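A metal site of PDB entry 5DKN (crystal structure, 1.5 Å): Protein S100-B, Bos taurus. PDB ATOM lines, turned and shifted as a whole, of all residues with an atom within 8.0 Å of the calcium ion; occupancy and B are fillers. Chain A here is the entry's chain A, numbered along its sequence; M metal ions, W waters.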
ATOM      1  N   PHE A  15       7.603   8.386   9.304  1.00  0.00           N
ATOM      2  CA  PHE A  15       8.231   8.246  10.619  1.00  0.00           C
ATOM      3  C   PHE A  15       7.210   7.869  11.678  1.00  0.00           C
ATOM      4  O   PHE A  15       7.395   6.896  12.416  1.00  0.00           O
ATOM      5  CB  PHE A  15       8.937   9.542  11.031  1.00  0.00           C
ATOM      6  CG  PHE A  15       9.633   9.444  12.384  1.00  0.00           C
ATOM      7  CD1 PHE A  15      10.870   8.820  12.501  1.00  0.00           C
ATOM      8  CD2 PHE A  15       9.034   9.958  13.531  1.00  0.00           C
ATOM      9  CE1 PHE A  15      11.510   8.739  13.736  1.00  0.00           C
ATOM     10  CE2 PHE A  15       9.663   9.871  14.772  1.00  0.00           C
ATOM     11  CZ  PHE A  15      10.910   9.256  14.870  1.00  0.00           C
ATOM     12  N   TYR A  18       5.527   4.413  11.933  1.00  0.00           N
ATOM     13  CA  TYR A  18       6.295   3.336  12.555  1.00  0.00           C
ATOM     14  C   TYR A  18       6.723   3.601  13.993  1.00  0.00           C
ATOM     15  O   TYR A  18       6.741   2.677  14.801  1.00  0.00           O
ATOM     16  CB  TYR A  18       7.488   2.934  11.657  1.00  0.00           C
ATOM     17  CG  TYR A  18       6.982   2.225  10.434  1.00  0.00           C
ATOM     18  CD1 TYR A  18       6.598   2.922   9.301  1.00  0.00           C
ATOM     19  CD2 TYR A  18       6.828   0.846  10.426  1.00  0.00           C
ATOM     20  CE1 TYR A  18       6.099   2.281   8.191  1.00  0.00           C
ATOM     21  CE2 TYR A  18       6.336   0.185   9.326  1.00  0.00           C
ATOM     22  CZ  TYR A  18       5.968   0.907   8.199  1.00  0.00           C
ATOM     23  OH  TYR A  18       5.475   0.259   7.094  1.00  0.00           O
ATOM     24  N   SER A  19       7.041   4.853  14.319  1.00  0.00           N
ATOM     25  CA  SER A  19       7.556   5.196  15.649  1.00  0.00           C
ATOM     26  C   SER A  19       6.526   5.001  16.757  1.00  0.00           C
ATOM     27  O   SER A  19       6.891   4.770  17.911  1.00  0.00           O
ATOM     28  CB  SER A  19       8.067   6.645  15.677  1.00  0.00           C
ATOM     29  OG  SER A  19       7.000   7.568  15.530  1.00  0.00           O
ATOM     30  N   GLY A  20       5.253   5.075  16.400  1.00  0.00           N
ATOM     31  CA  GLY A  20       4.193   5.012  17.405  1.00  0.00           C
ATOM     32  C   GLY A  20       3.744   3.619  17.792  1.00  0.00           C
ATOM     33  O   GLY A  20       2.956   3.469  18.734  1.00  0.00           O
ATOM     34  N   ARG A  21       4.222   2.602  17.080  1.00  0.00           N
ATOM     35  CA  ARG A  21       3.744   1.231  17.255  1.00  0.00           C
ATOM     36  C   ARG A  21       4.132   0.618  18.593  1.00  0.00           C
ATOM     37  O   ARG A  21       3.352  -0.114  19.198  1.00  0.00           O
ATOM     38  CB  ARG A  21       4.275   0.348  16.137  1.00  0.00           C
ATOM     39  CG  ARG A  21       3.776   0.782  14.778  1.00  0.00           C
ATOM     40  CD  ARG A  21       4.389   0.022  13.638  1.00  0.00           C
ATOM     41  NE  ARG A  21       3.666   0.367  12.418  1.00  0.00           N
ATOM     42  CZ  ARG A  21       3.368  -0.485  11.450  1.00  0.00           C
ATOM     43  NH1 ARG A  21       3.751  -1.761  11.529  1.00  0.00           N
ATOM     44  NH2 ARG A  21       2.688  -0.071  10.392  1.00  0.00           N
ATOM     45  N   GLU A  22       5.343   0.934  19.048  1.00  0.00           N
ATOM     46  CA  GLU A  22       5.900   0.359  20.258  1.00  0.00           C
ATOM     47  C   GLU A  22       6.627   1.391  21.097  1.00  0.00           C
ATOM     48  O   GLU A  22       7.265   2.308  20.547  1.00  0.00           O
ATOM     49  CB  GLU A  22       6.928  -0.715  19.905  1.00  0.00           C
ATOM     50  CG  GLU A  22       6.482  -1.793  18.963  1.00  0.00           C
ATOM     51  CD  GLU A  22       7.601  -2.749  18.682  1.00  0.00           C
ATOM     52  OE1 GLU A  22       8.009  -3.478  19.616  1.00  0.00           O
ATOM     53  OE2 GLU A  22       8.110  -2.744  17.545  1.00  0.00           O
ATOM     54  N   GLY A  23       6.574   1.202  22.410  1.00  0.00           N
ATOM     55  CA  GLY A  23       7.400   1.956  23.347  1.00  0.00           C
ATOM     56  C   GLY A  23       7.263   3.450  23.199  1.00  0.00           C
ATOM     57  O   GLY A  23       6.156   3.977  23.058  1.00  0.00           O
ATOM     58  N   ASP A  24       8.410   4.128  23.210  1.00  0.00           N
ATOM     59  CA  ASP A  24       8.461   5.558  22.935  1.00  0.00           C
ATOM     60  C   ASP A  24       7.776   5.867  21.601  1.00  0.00           C
ATOM     61  O   ASP A  24       8.199   5.379  20.548  1.00  0.00           O
ATOM     62  CB  ASP A  24       9.932   5.986  22.898  1.00  0.00           C
ATOM     63  CG  ASP A  24      10.095   7.489  22.931  1.00  0.00           C
ATOM     64  OD1 ASP A  24       9.303   8.193  22.283  1.00  0.00           O
ATOM     65  OD2 ASP A  24      11.031   7.957  23.605  1.00  0.00           O
ATOM     66  N   LYS A  25       6.724   6.673  21.642  1.00  0.00           N
ATOM     67  CA  LYS A  25       5.968   6.977  20.434  1.00  0.00           C
ATOM     68  C   LYS A  25       6.714   7.934  19.503  1.00  0.00           C
ATOM     69  O   LYS A  25       6.328   8.106  18.348  1.00  0.00           O
ATOM     70  CB  LYS A  25       4.581   7.532  20.787  1.00  0.00           C
ATOM     71  CG  LYS A  25       3.751   6.608  21.665  1.00  0.00           C
ATOM     72  CD  LYS A  25       2.531   7.337  22.204  1.00  0.00           C
ATOM     73  CE  LYS A  25       1.930   6.612  23.404  1.00  0.00           C
ATOM     74  NZ  LYS A  25       0.997   7.482  24.182  1.00  0.00           N
ATOM     75  N   HIS A  26       7.780   8.538  20.010  1.00  0.00           N
ATOM     76  CA  HIS A  26       8.536   9.534  19.250  1.00  0.00           C
ATOM     77  C   HIS A  26       9.846   9.012  18.673  1.00  0.00           C
ATOM     78  O   HIS A  26      10.602   9.772  18.070  1.00  0.00           O
ATOM     79  CB  HIS A  26       8.808  10.745  20.138  1.00  0.00           C
ATOM     80  CG  HIS A  26       7.584  11.325  20.748  1.00  0.00           C
ATOM     81  ND1 HIS A  26       6.611  11.965  20.003  1.00  0.00           N
ATOM     82  CD2 HIS A  26       7.147  11.356  22.039  1.00  0.00           C
ATOM     83  CE1 HIS A  26       5.646  12.370  20.798  1.00  0.00           C
ATOM     84  NE2 HIS A  26       5.942  12.019  22.033  1.00  0.00           N
ATOM     85  N   LYS A  27      10.128   7.731  18.858  1.00  0.00           N
ATOM     86  CA  LYS A  27      11.363   7.138  18.383  1.00  0.00           C
ATOM     87  C   LYS A  27      11.108   5.781  17.741  1.00  0.00           C
ATOM     88  O   LYS A  27      10.158   5.088  18.106  1.00  0.00           O
ATOM     89  CB  LYS A  27      12.373   6.982  19.533  1.00  0.00           C
ATOM     90  CG  LYS A  27      12.709   8.251  20.303  1.00  0.00           C
ATOM     91  CD  LYS A  27      13.705   7.966  21.412  1.00  0.00           C
ATOM     92  CE  LYS A  27      13.975   9.205  22.242  1.00  0.00           C
ATOM     93  NZ  LYS A  27      14.846   8.904  23.418  1.00  0.00           N
ATOM     94  N   LEU A  28      11.963   5.417  16.785  1.00  0.00           N
ATOM     95  CA  LEU A  28      11.964   4.090  16.214  1.00  0.00           C
ATOM     96  C   LEU A  28      12.933   3.185  16.984  1.00  0.00           C
ATOM     97  O   LEU A  28      14.145   3.436  16.983  1.00  0.00           O
ATOM     98  CB  LEU A  28      12.410   4.129  14.751  1.00  0.00           C
ATOM     99  CG  LEU A  28      11.615   4.966  13.758  1.00  0.00           C
ATOM    100  CD1 LEU A  28      12.477   5.212  12.509  1.00  0.00           C
ATOM    101  CD2 LEU A  28      10.319   4.266  13.388  1.00  0.00           C
ATOM    102  N   LYS A  29      12.412   2.142  17.621  1.00  0.00           N
ATOM    103  CA  LYS A  29      13.303   1.111  18.156  1.00  0.00           C
ATOM    104  C   LYS A  29      13.661   0.187  16.990  1.00  0.00           C
ATOM    105  O   LYS A  29      13.076   0.305  15.909  1.00  0.00           O
ATOM    106  CB  LYS A  29      12.662   0.361  19.321  1.00  0.00           C
ATOM    107  CG  LYS A  29      11.361  -0.331  18.982  1.00  0.00           C
ATOM    108  CD  LYS A  29      10.621  -0.778  20.253  1.00  0.00           C
ATOM    109  CE  LYS A  29      11.359  -1.882  20.972  1.00  0.00           C
ATOM    110  NZ  LYS A  29      11.000  -3.249  20.522  1.00  0.00           N
ATOM    111  N   LYS A  30      14.608  -0.717  17.197  1.00  0.00           N
ATOM    112  CA  LYS A  30      15.104  -1.570  16.111  1.00  0.00           C
ATOM    113  C   LYS A  30      13.991  -2.341  15.400  1.00  0.00           C
ATOM    114  O   LYS A  30      13.999  -2.461  14.168  1.00  0.00           O
ATOM    115  CB  LYS A  30      16.183  -2.527  16.622  1.00  0.00           C
ATOM    116  CG  LYS A  30      17.544  -1.856  16.821  1.00  0.00           C
ATOM    117  CD  LYS A  30      18.605  -2.865  17.245  1.00  0.00           C
ATOM    118  CE  LYS A  30      18.242  -3.492  18.586  1.00  0.00           C
ATOM    119  NZ  LYS A  30      18.332  -2.519  19.704  1.00  0.00           N
ATOM    120  N   SER A  31      13.030  -2.857  16.149  1.00  0.00           N
ATOM    121  CA  SER A  31      11.936  -3.601  15.532  1.00  0.00           C
ATOM    122  C   SER A  31      11.102  -2.737  14.593  1.00  0.00           C
ATOM    123  O   SER A  31      10.725  -3.198  13.511  1.00  0.00           O
ATOM    124  CB  SER A  31      11.059  -4.287  16.592  1.00  0.00           C
ATOM    125  OG  SER A  31      10.652  -3.395  17.620  1.00  0.00           O
ATOM    126  N   GLU A  32      10.838  -1.496  14.990  1.00  0.00           N
ATOM    127  CA  GLU A  32      10.102  -0.540  14.158  1.00  0.00           C
ATOM    128  C   GLU A  32      10.903  -0.131  12.926  1.00  0.00           C
ATOM    129  O   GLU A  32      10.376  -0.071  11.813  1.00  0.00           O
ATOM    130  CB  GLU A  32       9.743   0.689  14.988  1.00  0.00           C
ATOM    131  CG  GLU A  32       8.781   0.389  16.131  1.00  0.00           C
ATOM    132  CD  GLU A  32       8.629   1.543  17.086  1.00  0.00           C
ATOM    133  OE1 GLU A  32       9.626   2.260  17.319  1.00  0.00           O
ATOM    134  OE2 GLU A  32       7.523   1.751  17.608  1.00  0.00           O
ATOM    135  N   LEU A  33      12.195   0.127  13.128  1.00  0.00           N
ATOM    136  CA  LEU A  33      13.082   0.471  12.022  1.00  0.00           C
ATOM    137  C   LEU A  33      13.160  -0.650  10.983  1.00  0.00           C
ATOM    138  O   LEU A  33      13.145  -0.389   9.779  1.00  0.00           O
ATOM    139  CB  LEU A  33      14.475   0.803  12.562  1.00  0.00           C
ATOM    140  CG  LEU A  33      15.544   1.105  11.518  1.00  0.00           C
ATOM    141  CD1 LEU A  33      15.205   2.392  10.795  1.00  0.00           C
ATOM    142  CD2 LEU A  33      16.913   1.213  12.182  1.00  0.00           C
ATOM    143  N   GLU A  68      17.872   3.827  19.902  1.00  0.00           N
ATOM    144  CA  GLU A  68      16.718   4.107  19.068  1.00  0.00           C
ATOM    145  C   GLU A  68      17.030   5.226  18.094  1.00  0.00           C
ATOM    146  O   GLU A  68      18.006   5.951  18.248  1.00  0.00           O
ATOM    147  CB  GLU A  68      15.507   4.468  19.927  1.00  0.00           C
ATOM    148  CG  GLU A  68      15.143   3.397  20.953  1.00  0.00           C
ATOM    149  CD  GLU A  68      13.681   3.411  21.349  1.00  0.00           C
ATOM    150  OE1 GLU A  68      12.862   3.896  20.549  1.00  0.00           O
ATOM    151  OE2 GLU A  68      13.359   2.922  22.461  1.00  0.00           O
ATOM    152  N   CYS A  69      16.181   5.351  17.075  1.00  0.00           N
ATOM    153  CA  CYS A  69      16.316   6.386  16.085  1.00  0.00           C
ATOM    154  C   CYS A  69      15.220   7.449  16.269  1.00  0.00           C
ATOM    155  O   CYS A  69      14.046   7.188  15.989  1.00  0.00           O
ATOM    156  CB  CYS A  69      16.253   5.771  14.688  1.00  0.00           C
ATOM    157  SG  CYS A  69      16.395   6.940  13.323  1.00  0.00           S
HETATM  158 CA    CA M   1       8.556   3.604  19.055  1.00  0.00          CA
HETATM  159  O   HOH W   1      10.317   2.809  20.336  1.00  0.00           O
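The calcium ion is bound by water W1, at 2.3 Å. The calcium ion is bound by the backbone carbonyl oxygen (O) of Ser 19, 2.3 Å away. The calcium ion is bound by the backbone carbonyl oxygen (O) of Asp 24 (2.3 Å). O of Glu 22 binds the calcium ion (2.4 Å). O of Lys 27 binds the calcium ion (2.4 Å). The calcium ion is bound by OE1 of Glu 32, 2.4 Å away. OE2 of Glu 32 binds the calcium ion, 2.6 Å away. The calcium ion has seven donor atoms within binding distance.
Water W1 lies within hydrogen-bond range of the side-chain carboxylate (OE1) of Glu 68 (2.8 Å) and the backbone NH (N) of Lys 29 (3.5 Å).
OG of Ser 19 lies within hydrogen-bond range of O of Phe 15 (3.2 Å). NZ of Lys 29 lies within salt-bridge range of OE1 of Glu 22 (3.1 Å). The side-chain carboxylate (OE1) of Glu 32 sits close to the backbone NH (N) of Lys 29, 2.8 Å away. OD2 of Asp 24 lies within salt-bridge range of NZ of Lys 27, 3.9 Å away. OD1 of Asp 24 lies within hydrogen-bond range of N of His 26 (2.8 Å). The side-chain hydroxyl (OG) of Ser 19 is in hydrogen-bond range of the backbone carbonyl oxygen (O) of Lys 25 (2.9 Å). The side-chain carboxylate (OE2) of Glu 32 sits close to the backbone NH (N) of Arg 21, at 3.4 Å. The side-chain hydroxyl of Ser 31 lies within hydrogen-bond range of the side-chain carboxylate of Glu 22.
Of the 19 residues printed, 5 come within 4 Å of the calcium ion.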
